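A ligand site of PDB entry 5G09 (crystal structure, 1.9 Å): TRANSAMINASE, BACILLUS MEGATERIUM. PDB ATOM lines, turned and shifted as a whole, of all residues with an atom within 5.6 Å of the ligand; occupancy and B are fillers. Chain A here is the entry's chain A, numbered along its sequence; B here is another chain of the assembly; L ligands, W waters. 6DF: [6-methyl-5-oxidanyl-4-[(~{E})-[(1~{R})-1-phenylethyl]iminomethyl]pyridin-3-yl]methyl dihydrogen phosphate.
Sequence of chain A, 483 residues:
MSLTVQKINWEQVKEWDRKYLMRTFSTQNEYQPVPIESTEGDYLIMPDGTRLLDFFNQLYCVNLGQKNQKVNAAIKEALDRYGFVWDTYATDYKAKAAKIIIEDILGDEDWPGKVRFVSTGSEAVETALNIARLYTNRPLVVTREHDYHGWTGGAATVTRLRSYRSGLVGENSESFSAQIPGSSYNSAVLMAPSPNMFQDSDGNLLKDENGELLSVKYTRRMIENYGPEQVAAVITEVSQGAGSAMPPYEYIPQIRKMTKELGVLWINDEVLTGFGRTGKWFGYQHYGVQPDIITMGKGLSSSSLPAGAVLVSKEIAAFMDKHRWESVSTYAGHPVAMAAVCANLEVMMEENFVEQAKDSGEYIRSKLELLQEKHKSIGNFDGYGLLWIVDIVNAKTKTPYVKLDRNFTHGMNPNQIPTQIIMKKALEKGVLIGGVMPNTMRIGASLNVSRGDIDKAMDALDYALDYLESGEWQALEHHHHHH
The backbone NH (N) of Ser 122 sits at hydrogen-bond distance from an oxygen (O3P) of the ligand (2.8 Å). An oxygen (O2P) of the ligand is in hydrogen-bond range of the backbone NH (N) of Thr 330 of chain B (2.7 Å). O2P of the ligand is in hydrogen-bond range of OG1 of Thr 330 of chain B, 2.7 Å away. N of Gly 121 sits at hydrogen-bond distance from O1P of the ligand (2.9 Å). The side-chain carboxylate of Asp 269 lies within hydrogen-bond range of a nitrogen (N1) of the ligand (2.8 Å). An oxygen (O3P) of the ligand lies within hydrogen-bond range of the side-chain hydroxyl (OG) of Ser 122, 2.6 Å away.
The side-chain hydroxyl (OG1) of Thr 330 of chain B lies within hydrogen-bond range of the side-chain amino group (NZ) of Lys 298 (3.1 Å). N of Val 271 is in hydrogen-bond range of OD1 of Asp 269, at 2.9 Å. The side-chain hydroxyl (OG1) of Thr 120 lies within hydrogen-bond range of the backbone NH (N) of Glu 123 of chain A. O of Val 328 of chain B is in hydrogen-bond range of OH of Tyr 148 (3.3 Å). NZ of Lys 298 lies within hydrogen-bond range of O of Leu 59. The side-chain hydroxyl (OG) of Ser 329 of chain B sits close to the indole nitrogen (NE1) of Trp 151 (3.5 Å). The backbone NH of Tyr 148 lies within hydrogen-bond range of the side-chain carboxylate of Glu 237 (2.9 Å). The side-chain hydroxyl (OG1) of Thr 120 is in hydrogen-bond range of the side-chain carboxylate (OE2) of Glu 123 of chain B, 2.9 Å away.
Leu 59 touches the ligand (CD1 to C8, 3.7 Å). CD2 of Tyr 60 touches C11 of the ligand, 3.8 Å away. Thr 120 touches the ligand (CB to O1P, 3.9 Å). CE2 of Tyr 148 touches N2 of the ligand, at 3.1 Å. His 149 touches the ligand (C to C6, 3.5 Å). Gly 150 touches the ligand. OE1 of Glu 237 touches C2' of the ligand, at 3.4 Å. Ala 242 touches the ligand (CB to C12, 3.7 Å). Val 271 touches the ligand. Leu 272 touches the ligand (CD1 to O3, 3.7 Å). Lys 298 touches the ligand. CG1 of Val 328 of chain B touches C14 of the ligand (3.97 Å). Ser 329 of chain B touches the ligand (C to O2P, 3.7 Å). Of the 25 residues printed, 17 come within 4 Å of the ligand.
Water W3 lies within hydrogen-bond range of OG of Ser 329 of chain B, OE2 of Glu 123 of chain B, O3P of the ligand and NE1 of Trp 151. Water W5 lies within hydrogen-bond range of O3 of the ligand (2.7 Å), N of Ala 242 (2.8 Å) and OE1 of Glu 237 (2.8 Å). Water W6 lies within hydrogen-bond range of O1P of the ligand, N of Tyr 331 of chain B and N of Thr 330 of chain B. Water W4 lies within hydrogen-bond range of the side-chain hydroxyl (OH) of Tyr 148, the backbone carbonyl oxygen (O) of Val 328 of chain B and an oxygen (O2P) of the ligand. Water W2 lies within hydrogen-bond range of O1P of the ligand (2.8 Å) and N of Lys 298 (3.0 Å).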
ATOM      1  N   LEU A  59      10.225   2.528  19.390  1.00  0.00           N
ATOM      2  CA  LEU A  59       9.221   3.548  19.103  1.00  0.00           C
ATOM      3  C   LEU A  59       9.168   3.767  17.596  1.00  0.00           C
ATOM      4  O   LEU A  59       9.120   4.889  17.109  1.00  0.00           O
ATOM      5  CB  LEU A  59       9.488   4.841  19.903  1.00  0.00           C
ATOM      6  CG  LEU A  59       9.346   4.814  21.439  1.00  0.00           C
ATOM      7  CD1 LEU A  59       9.961   6.062  22.094  1.00  0.00           C
ATOM      8  CD2 LEU A  59       7.878   4.656  21.861  1.00  0.00           C
ATOM      9  N   TYR A  60       9.156   2.645  16.849  1.00  0.00           N
ATOM     10  CA  TYR A  60       9.046   2.682  15.391  1.00  0.00           C
ATOM     11  C   TYR A  60      10.240   3.437  14.861  1.00  0.00           C
ATOM     12  O   TYR A  60      10.142   4.195  13.904  1.00  0.00           O
ATOM     13  CB  TYR A  60       7.676   3.256  14.914  1.00  0.00           C
ATOM     14  CG  TYR A  60       6.562   2.607  15.696  1.00  0.00           C
ATOM     15  CD1 TYR A  60       6.079   1.340  15.330  1.00  0.00           C
ATOM     16  CD2 TYR A  60       6.052   3.199  16.851  1.00  0.00           C
ATOM     17  CE1 TYR A  60       5.113   0.694  16.096  1.00  0.00           C
ATOM     18  CE2 TYR A  60       5.093   2.562  17.626  1.00  0.00           C
ATOM     19  CZ  TYR A  60       4.619   1.309  17.234  1.00  0.00           C
ATOM     20  OH  TYR A  60       3.681   0.678  18.007  1.00  0.00           O
ATOM     21  N   THR A 120      16.730  15.863  18.191  1.00  0.00           N
ATOM     22  CA  THR A 120      15.528  15.092  18.461  1.00  0.00           C
ATOM     23  C   THR A 120      14.414  15.448  17.501  1.00  0.00           C
ATOM     24  O   THR A 120      14.465  16.463  16.829  1.00  0.00           O
ATOM     25  CB  THR A 120      14.985  15.280  19.915  1.00  0.00           C
ATOM     26  OG1 THR A 120      14.438  16.607  20.077  1.00  0.00           O
ATOM     27  CG2 THR A 120      16.067  15.028  20.953  1.00  0.00           C
ATOM     28  N   GLY A 121      13.395  14.603  17.455  1.00  0.00           N
ATOM     29  CA  GLY A 121      12.245  14.869  16.578  1.00  0.00           C
ATOM     30  C   GLY A 121      11.469  16.103  17.022  1.00  0.00           C
ATOM     31  O   GLY A 121      11.006  16.894  16.173  1.00  0.00           O
ATOM     32  N   SER A 122      11.288  16.266  18.347  1.00  0.00           N
ATOM     33  CA  SER A 122      10.569  17.458  18.873  1.00  0.00           C
ATOM     34  C   SER A 122      11.338  18.733  18.506  1.00  0.00           C
ATOM     35  O   SER A 122      10.760  19.749  18.137  1.00  0.00           O
ATOM     36  CB  SER A 122      10.394  17.383  20.396  1.00  0.00           C
ATOM     37  OG  SER A 122       9.592  16.309  20.797  1.00  0.00           O
ATOM     38  N   GLU A 123      12.676  18.695  18.622  1.00  0.00           N
ATOM     39  CA  GLU A 123      13.505  19.833  18.194  1.00  0.00           C
ATOM     40  C   GLU A 123      13.329  20.110  16.707  1.00  0.00           C
ATOM     41  O   GLU A 123      13.310  21.250  16.276  1.00  0.00           O
ATOM     42  CB  GLU A 123      14.994  19.643  18.583  1.00  0.00           C
ATOM     43  CG  GLU A 123      15.232  19.767  20.089  1.00  0.00           C
ATOM     44  CD  GLU A 123      16.691  19.907  20.498  1.00  0.00           C
ATOM     45  OE1 GLU A 123      17.576  19.575  19.687  1.00  0.00           O
ATOM     46  OE2 GLU A 123      16.956  20.379  21.650  1.00  0.00           O
ATOM     47  N   VAL A 125      10.622  19.489  14.922  1.00  0.00           N
ATOM     48  CA  VAL A 125       9.301  20.125  14.781  1.00  0.00           C
ATOM     49  C   VAL A 125       9.347  21.594  15.259  1.00  0.00           C
ATOM     50  O   VAL A 125       8.815  22.485  14.604  1.00  0.00           O
ATOM     51  CB  VAL A 125       8.186  19.311  15.476  1.00  0.00           C
ATOM     52  CG1 VAL A 125       6.875  20.113  15.556  1.00  0.00           C
ATOM     53  CG2 VAL A 125       7.962  18.006  14.733  1.00  0.00           C
ATOM     54  N   TYR A 148       0.398  13.652  16.757  1.00  0.00           N
ATOM     55  CA  TYR A 148       1.504  13.709  17.716  1.00  0.00           C
ATOM     56  C   TYR A 148       2.721  14.296  16.988  1.00  0.00           C
ATOM     57  O   TYR A 148       3.201  13.712  15.980  1.00  0.00           O
ATOM     58  CB  TYR A 148       1.838  12.318  18.310  1.00  0.00           C
ATOM     59  CG  TYR A 148       2.871  12.482  19.417  1.00  0.00           C
ATOM     60  CD1 TYR A 148       2.471  12.899  20.688  1.00  0.00           C
ATOM     61  CD2 TYR A 148       4.249  12.313  19.183  1.00  0.00           C
ATOM     62  CE1 TYR A 148       3.387  13.131  21.693  1.00  0.00           C
ATOM     63  CE2 TYR A 148       5.186  12.524  20.196  1.00  0.00           C
ATOM     64  CZ  TYR A 148       4.749  12.937  21.451  1.00  0.00           C
ATOM     65  OH  TYR A 148       5.664  13.179  22.484  1.00  0.00           O
ATOM     66  N   HIS A 149       3.209  15.446  17.449  1.00  0.00           N
ATOM     67  CA  HIS A 149       4.386  16.039  16.840  1.00  0.00           C
ATOM     68  C   HIS A 149       5.531  16.316  17.834  1.00  0.00           C
ATOM     69  O   HIS A 149       6.419  17.091  17.534  1.00  0.00           O
ATOM     70  CB  HIS A 149       3.981  17.338  16.124  1.00  0.00           C
ATOM     71  CG  HIS A 149       2.991  17.136  15.001  1.00  0.00           C
ATOM     72  ND1 HIS A 149       3.333  16.498  13.819  1.00  0.00           N
ATOM     73  CD2 HIS A 149       1.678  17.473  14.884  1.00  0.00           C
ATOM     74  CE1 HIS A 149       2.273  16.447  13.034  1.00  0.00           C
ATOM     75  NE2 HIS A 149       1.253  17.030  13.641  1.00  0.00           N
ATOM     76  N   GLY A 150       5.482  15.722  19.024  1.00  0.00           N
ATOM     77  CA  GLY A 150       6.532  15.911  20.032  1.00  0.00           C
ATOM     78  C   GLY A 150       5.997  16.493  21.327  1.00  0.00           C
ATOM     79  O   GLY A 150       4.769  16.681  21.484  1.00  0.00           O
ATOM     80  N   TRP A 151       6.902  16.757  22.274  1.00  0.00           N
ATOM     81  CA  TRP A 151       6.512  16.991  23.666  1.00  0.00           C
ATOM     82  C   TRP A 151       7.002  18.318  24.185  1.00  0.00           C
ATOM     83  O   TRP A 151       6.512  18.789  25.190  1.00  0.00           O
ATOM     84  CB  TRP A 151       7.043  15.876  24.584  1.00  0.00           C
ATOM     85  CG  TRP A 151       8.566  15.870  24.666  1.00  0.00           C
ATOM     86  CD1 TRP A 151       9.423  15.198  23.821  1.00  0.00           C
ATOM     87  CD2 TRP A 151       9.383  16.580  25.588  1.00  0.00           C
ATOM     88  NE1 TRP A 151      10.708  15.447  24.176  1.00  0.00           N
ATOM     89  CE2 TRP A 151      10.723  16.278  25.269  1.00  0.00           C
ATOM     90  CE3 TRP A 151       9.108  17.400  26.700  1.00  0.00           C
ATOM     91  CZ2 TRP A 151      11.812  16.769  26.011  1.00  0.00           C
ATOM     92  CZ3 TRP A 151      10.207  17.933  27.431  1.00  0.00           C
ATOM     93  CH2 TRP A 151      11.542  17.611  27.077  1.00  0.00           C
ATOM     94  N   TYR A 164      -0.985  11.959  25.561  1.00  0.00           N
ATOM     95  CA  TYR A 164       0.459  12.147  25.372  1.00  0.00           C
ATOM     96  C   TYR A 164       0.929  13.604  25.465  1.00  0.00           C
ATOM     97  O   TYR A 164       1.890  14.006  24.795  1.00  0.00           O
ATOM     98  CB  TYR A 164       0.908  11.538  24.030  1.00  0.00           C
ATOM     99  CG  TYR A 164       1.035  10.052  24.130  1.00  0.00           C
ATOM    100  CD1 TYR A 164      -0.057   9.212  23.893  1.00  0.00           C
ATOM    101  CD2 TYR A 164       2.267   9.476  24.495  1.00  0.00           C
ATOM    102  CE1 TYR A 164       0.070   7.840  24.017  1.00  0.00           C
ATOM    103  CE2 TYR A 164       2.398   8.110  24.635  1.00  0.00           C
ATOM    104  CZ  TYR A 164       1.307   7.297  24.413  1.00  0.00           C
ATOM    105  OH  TYR A 164       1.464   5.954  24.539  1.00  0.00           O
ATOM    106  N   GLU A 237       0.760  14.340   9.663  1.00  0.00           N
ATOM    107  CA  GLU A 237       1.448  13.032   9.576  1.00  0.00           C
ATOM    108  C   GLU A 237       0.669  12.300   8.466  1.00  0.00           C
ATOM    109  O   GLU A 237      -0.568  12.313   8.528  1.00  0.00           O
ATOM    110  CB  GLU A 237       1.290  12.217  10.871  1.00  0.00           C
ATOM    111  CG  GLU A 237       1.849  12.843  12.141  1.00  0.00           C
ATOM    112  CD  GLU A 237       1.481  12.072  13.383  1.00  0.00           C
ATOM    113  OE1 GLU A 237       2.134  11.040  13.652  1.00  0.00           O
ATOM    114  OE2 GLU A 237       0.515  12.447  14.091  1.00  0.00           O
ATOM    115  N   GLY A 241       1.010   8.450  13.746  1.00  0.00           N
ATOM    116  CA  GLY A 241       1.877   7.421  14.310  1.00  0.00           C
ATOM    117  C   GLY A 241       1.336   6.986  15.676  1.00  0.00           C
ATOM    118  O   GLY A 241       0.692   5.927  15.798  1.00  0.00           O
ATOM    119  N   ALA A 242       1.584   7.806  16.707  1.00  0.00           N
ATOM    120  CA  ALA A 242       1.035   7.508  18.035  1.00  0.00           C
ATOM    121  C   ALA A 242      -0.481   7.438  17.951  1.00  0.00           C
ATOM    122  O   ALA A 242      -1.107   6.548  18.537  1.00  0.00           O
ATOM    123  CB  ALA A 242       1.468   8.571  19.036  1.00  0.00           C
ATOM    124  N   ASP A 269       5.224  15.988   8.785  1.00  0.00           N
ATOM    125  CA  ASP A 269       6.061  15.470   9.843  1.00  0.00           C
ATOM    126  C   ASP A 269       6.427  14.040   9.490  1.00  0.00           C
ATOM    127  O   ASP A 269       5.584  13.164   9.552  1.00  0.00           O
ATOM    128  CB  ASP A 269       5.304  15.519  11.193  1.00  0.00           C
ATOM    129  CG  ASP A 269       6.185  15.140  12.376  1.00  0.00           C
ATOM    130  OD1 ASP A 269       7.279  14.557  12.164  1.00  0.00           O
ATOM    131  OD2 ASP A 269       5.783  15.453  13.520  1.00  0.00           O
ATOM    132  N   VAL A 271       8.953  12.388  11.074  1.00  0.00           N
ATOM    133  CA  VAL A 271       9.795  11.852  12.124  1.00  0.00           C
ATOM    134  C   VAL A 271       9.612  10.328  12.244  1.00  0.00           C
ATOM    135  O   VAL A 271      10.585   9.573  12.361  1.00  0.00           O
ATOM    136  CB  VAL A 271       9.608  12.591  13.487  1.00  0.00           C
ATOM    137  CG1 VAL A 271      10.228  11.821  14.654  1.00  0.00           C
ATOM    138  CG2 VAL A 271      10.239  13.968  13.396  1.00  0.00           C
ATOM    139  N   LEU A 272       8.364   9.886  12.182  1.00  0.00           N
ATOM    140  CA  LEU A 272       8.085   8.472  12.324  1.00  0.00           C
ATOM    141  C   LEU A 272       7.983   7.749  10.946  1.00  0.00           C
ATOM    142  O   LEU A 272       8.475   6.616  10.794  1.00  0.00           O
ATOM    143  CB  LEU A 272       6.786   8.278  13.181  1.00  0.00           C
ATOM    144  CG  LEU A 272       6.421   6.855  13.607  1.00  0.00           C
ATOM    145  CD1 LEU A 272       5.798   6.850  15.014  1.00  0.00           C
ATOM    146  CD2 LEU A 272       5.456   6.180  12.613  1.00  0.00           C
ATOM    147  N   LYS A 298      14.169   9.637  14.497  1.00  0.00           N
ATOM    148  CA  LYS A 298      13.981   8.181  14.508  1.00  0.00           C
ATOM    149  C   LYS A 298      14.852   7.464  13.432  1.00  0.00           C
ATOM    150  O   LYS A 298      16.072   7.342  13.591  1.00  0.00           O
ATOM    151  CB  LYS A 298      12.472   7.846  14.394  1.00  0.00           C
ATOM    152  CG  LYS A 298      11.655   8.268  15.645  1.00  0.00           C
ATOM    153  CD  LYS A 298      10.161   8.128  15.425  1.00  0.00           C
ATOM    154  CE  LYS A 298       9.365   8.767  16.547  1.00  0.00           C
ATOM    155  NZ  LYS A 298       9.373   7.893  17.719  1.00  0.00           N
ATOM    156  N   VAL A 436      -0.453   1.591  21.179  1.00  0.00           N
ATOM    157  CA  VAL A 436      -0.473   2.645  22.199  1.00  0.00           C
ATOM    158  C   VAL A 436      -1.847   3.231  22.404  1.00  0.00           C
ATOM    159  O   VAL A 436      -2.100   3.836  23.460  1.00  0.00           O
ATOM    160  CB  VAL A 436       0.541   3.788  21.877  1.00  0.00           C
ATOM    161  CG1 VAL A 436       1.962   3.235  21.968  1.00  0.00           C
ATOM    162  CG2 VAL A 436       0.296   4.379  20.505  1.00  0.00           C
ATOM    163  N   GLU B 123      15.796  20.824  26.253  1.00  0.00           N
ATOM    164  CA  GLU B 123      14.858  19.791  26.708  1.00  0.00           C
ATOM    165  C   GLU B 123      14.808  19.672  28.231  1.00  0.00           C
ATOM    166  O   GLU B 123      13.716  19.439  28.811  1.00  0.00           O
ATOM    167  CB  GLU B 123      15.133  18.426  26.035  1.00  0.00           C
ATOM    168  CG  GLU B 123      14.664  18.416  24.587  1.00  0.00           C
ATOM    169  CD  GLU B 123      14.738  17.045  23.955  1.00  0.00           C
ATOM    170  OE1 GLU B 123      15.448  16.174  24.520  1.00  0.00           O
ATOM    171  OE2 GLU B 123      14.082  16.843  22.919  1.00  0.00           O
ATOM    172  N   VAL B 328       6.649  11.388  26.837  1.00  0.00           N
ATOM    173  CA  VAL B 328       7.644  10.532  26.173  1.00  0.00           C
ATOM    174  C   VAL B 328       8.551  11.366  25.269  1.00  0.00           C
ATOM    175  O   VAL B 328       8.070  12.269  24.567  1.00  0.00           O
ATOM    176  CB  VAL B 328       6.938   9.363  25.431  1.00  0.00           C
ATOM    177  CG1 VAL B 328       6.077   9.871  24.275  1.00  0.00           C
ATOM    178  CG2 VAL B 328       7.957   8.343  24.903  1.00  0.00           C
ATOM    179  N   SER B 329       9.851  11.060  25.278  1.00  0.00           N
ATOM    180  CA  SER B 329      10.864  11.661  24.411  1.00  0.00           C
ATOM    181  C   SER B 329      11.625  10.466  23.839  1.00  0.00           C
ATOM    182  O   SER B 329      12.192   9.677  24.620  1.00  0.00           O
ATOM    183  CB  SER B 329      11.815  12.528  25.262  1.00  0.00           C
ATOM    184  OG  SER B 329      12.966  12.858  24.517  1.00  0.00           O
ATOM    185  N   THR B 330      11.648  10.300  22.525  1.00  0.00           N
ATOM    186  CA  THR B 330      12.244   9.051  21.971  1.00  0.00           C
ATOM    187  C   THR B 330      13.650   8.769  22.579  1.00  0.00           C
ATOM    188  O   THR B 330      13.893   7.694  23.161  1.00  0.00           O
ATOM    189  CB  THR B 330      12.296   9.098  20.436  1.00  0.00           C
ATOM    190  OG1 THR B 330      10.981   9.315  19.911  1.00  0.00           O
ATOM    191  CG2 THR B 330      12.893   7.790  19.840  1.00  0.00           C
ATOM    192  N   TYR B 331      14.564   9.733  22.458  1.00  0.00           N
ATOM    193  CA  TYR B 331      15.980   9.537  22.865  1.00  0.00           C
ATOM    194  C   TYR B 331      16.278   9.773  24.357  1.00  0.00           C
ATOM    195  O   TYR B 331      17.444   9.674  24.770  1.00  0.00           O
ATOM    196  CB  TYR B 331      16.919  10.391  21.960  1.00  0.00           C
ATOM    197  CG  TYR B 331      16.795   9.973  20.484  1.00  0.00           C
ATOM    198  CD1 TYR B 331      16.650   8.623  20.163  1.00  0.00           C
ATOM    199  CD2 TYR B 331      16.808  10.902  19.432  1.00  0.00           C
ATOM    200  CE1 TYR B 331      16.504   8.187  18.847  1.00  0.00           C
ATOM    201  CE2 TYR B 331      16.689  10.467  18.104  1.00  0.00           C
ATOM    202  CZ  TYR B 331      16.547   9.098  17.832  1.00  0.00           C
ATOM    203  OH  TYR B 331      16.416   8.584  16.577  1.00  0.00           O
HETATM  204  N1  6DF L   1       6.810  13.597  15.348  1.00  0.00           N
HETATM  205  C2  6DF L   1       6.269  12.375  15.316  1.00  0.00           C
HETATM  206  N2  6DF L   1       6.731  10.140  18.946  1.00  0.00           N
HETATM  207  C3  6DF L   1       6.531  11.495  16.352  1.00  0.00           C
HETATM  208  C4  6DF L   1       7.395  11.863  17.397  1.00  0.00           C
HETATM  209  C5  6DF L   1       7.936  13.146  17.390  1.00  0.00           C
HETATM  210  C6  6DF L   1       7.636  13.997  16.348  1.00  0.00           C
HETATM  211  C7  6DF L   1       6.649   9.274  20.148  1.00  0.00           C
HETATM  212  C8  6DF L   1       7.952   8.954  20.828  1.00  0.00           C
HETATM  213  C9  6DF L   1       5.732   8.116  20.011  1.00  0.00           C
HETATM  214  C10 6DF L   1       5.655   7.393  18.808  1.00  0.00           C
HETATM  215  C11 6DF L   1       4.784   6.302  18.700  1.00  0.00           C
HETATM  216  C12 6DF L   1       4.006   5.932  19.811  1.00  0.00           C
HETATM  217  C13 6DF L   1       4.081   6.663  21.017  1.00  0.00           C
HETATM  218  O2P 6DF L   1      10.528  11.920  20.635  1.00  0.00           O
HETATM  219  P   6DF L   1      11.152  12.916  19.641  1.00  0.00           P
HETATM  220  O3P 6DF L   1      11.204  14.281  20.339  1.00  0.00           O
HETATM  221  O1P 6DF L   1      12.482  12.435  19.154  1.00  0.00           O
HETATM  222  O4P 6DF L   1      10.157  13.041  18.402  1.00  0.00           O
HETATM  223  C5' 6DF L   1       8.855  13.670  18.502  1.00  0.00           C
HETATM  224  C2' 6DF L   1       5.380  11.982  14.154  1.00  0.00           C
HETATM  225  O3  6DF L   1       5.959  10.253  16.346  1.00  0.00           O
HETATM  226  C4' 6DF L   1       7.646  10.955  18.570  1.00  0.00           C
HETATM  227  C14 6DF L   1       4.936   7.757  21.109  1.00  0.00           C
HETATM  228  O   HOH W   1       6.004  10.810  10.919  1.00  0.00           O
HETATM  229  O   HOH W   2      13.664  10.852  17.204  1.00  0.00           O
HETATM  230  O   HOH W   3      12.811  14.543  22.493  1.00  0.00           O
HETATM  231  O   HOH W   4       8.162  12.686  21.863  1.00  0.00           O
HETATM  232  O   HOH W   5       3.258   9.955  16.027  1.00  0.00           O
HETATM  233  O   HOH W   6      14.255  12.214  21.234  1.00  0.00           O
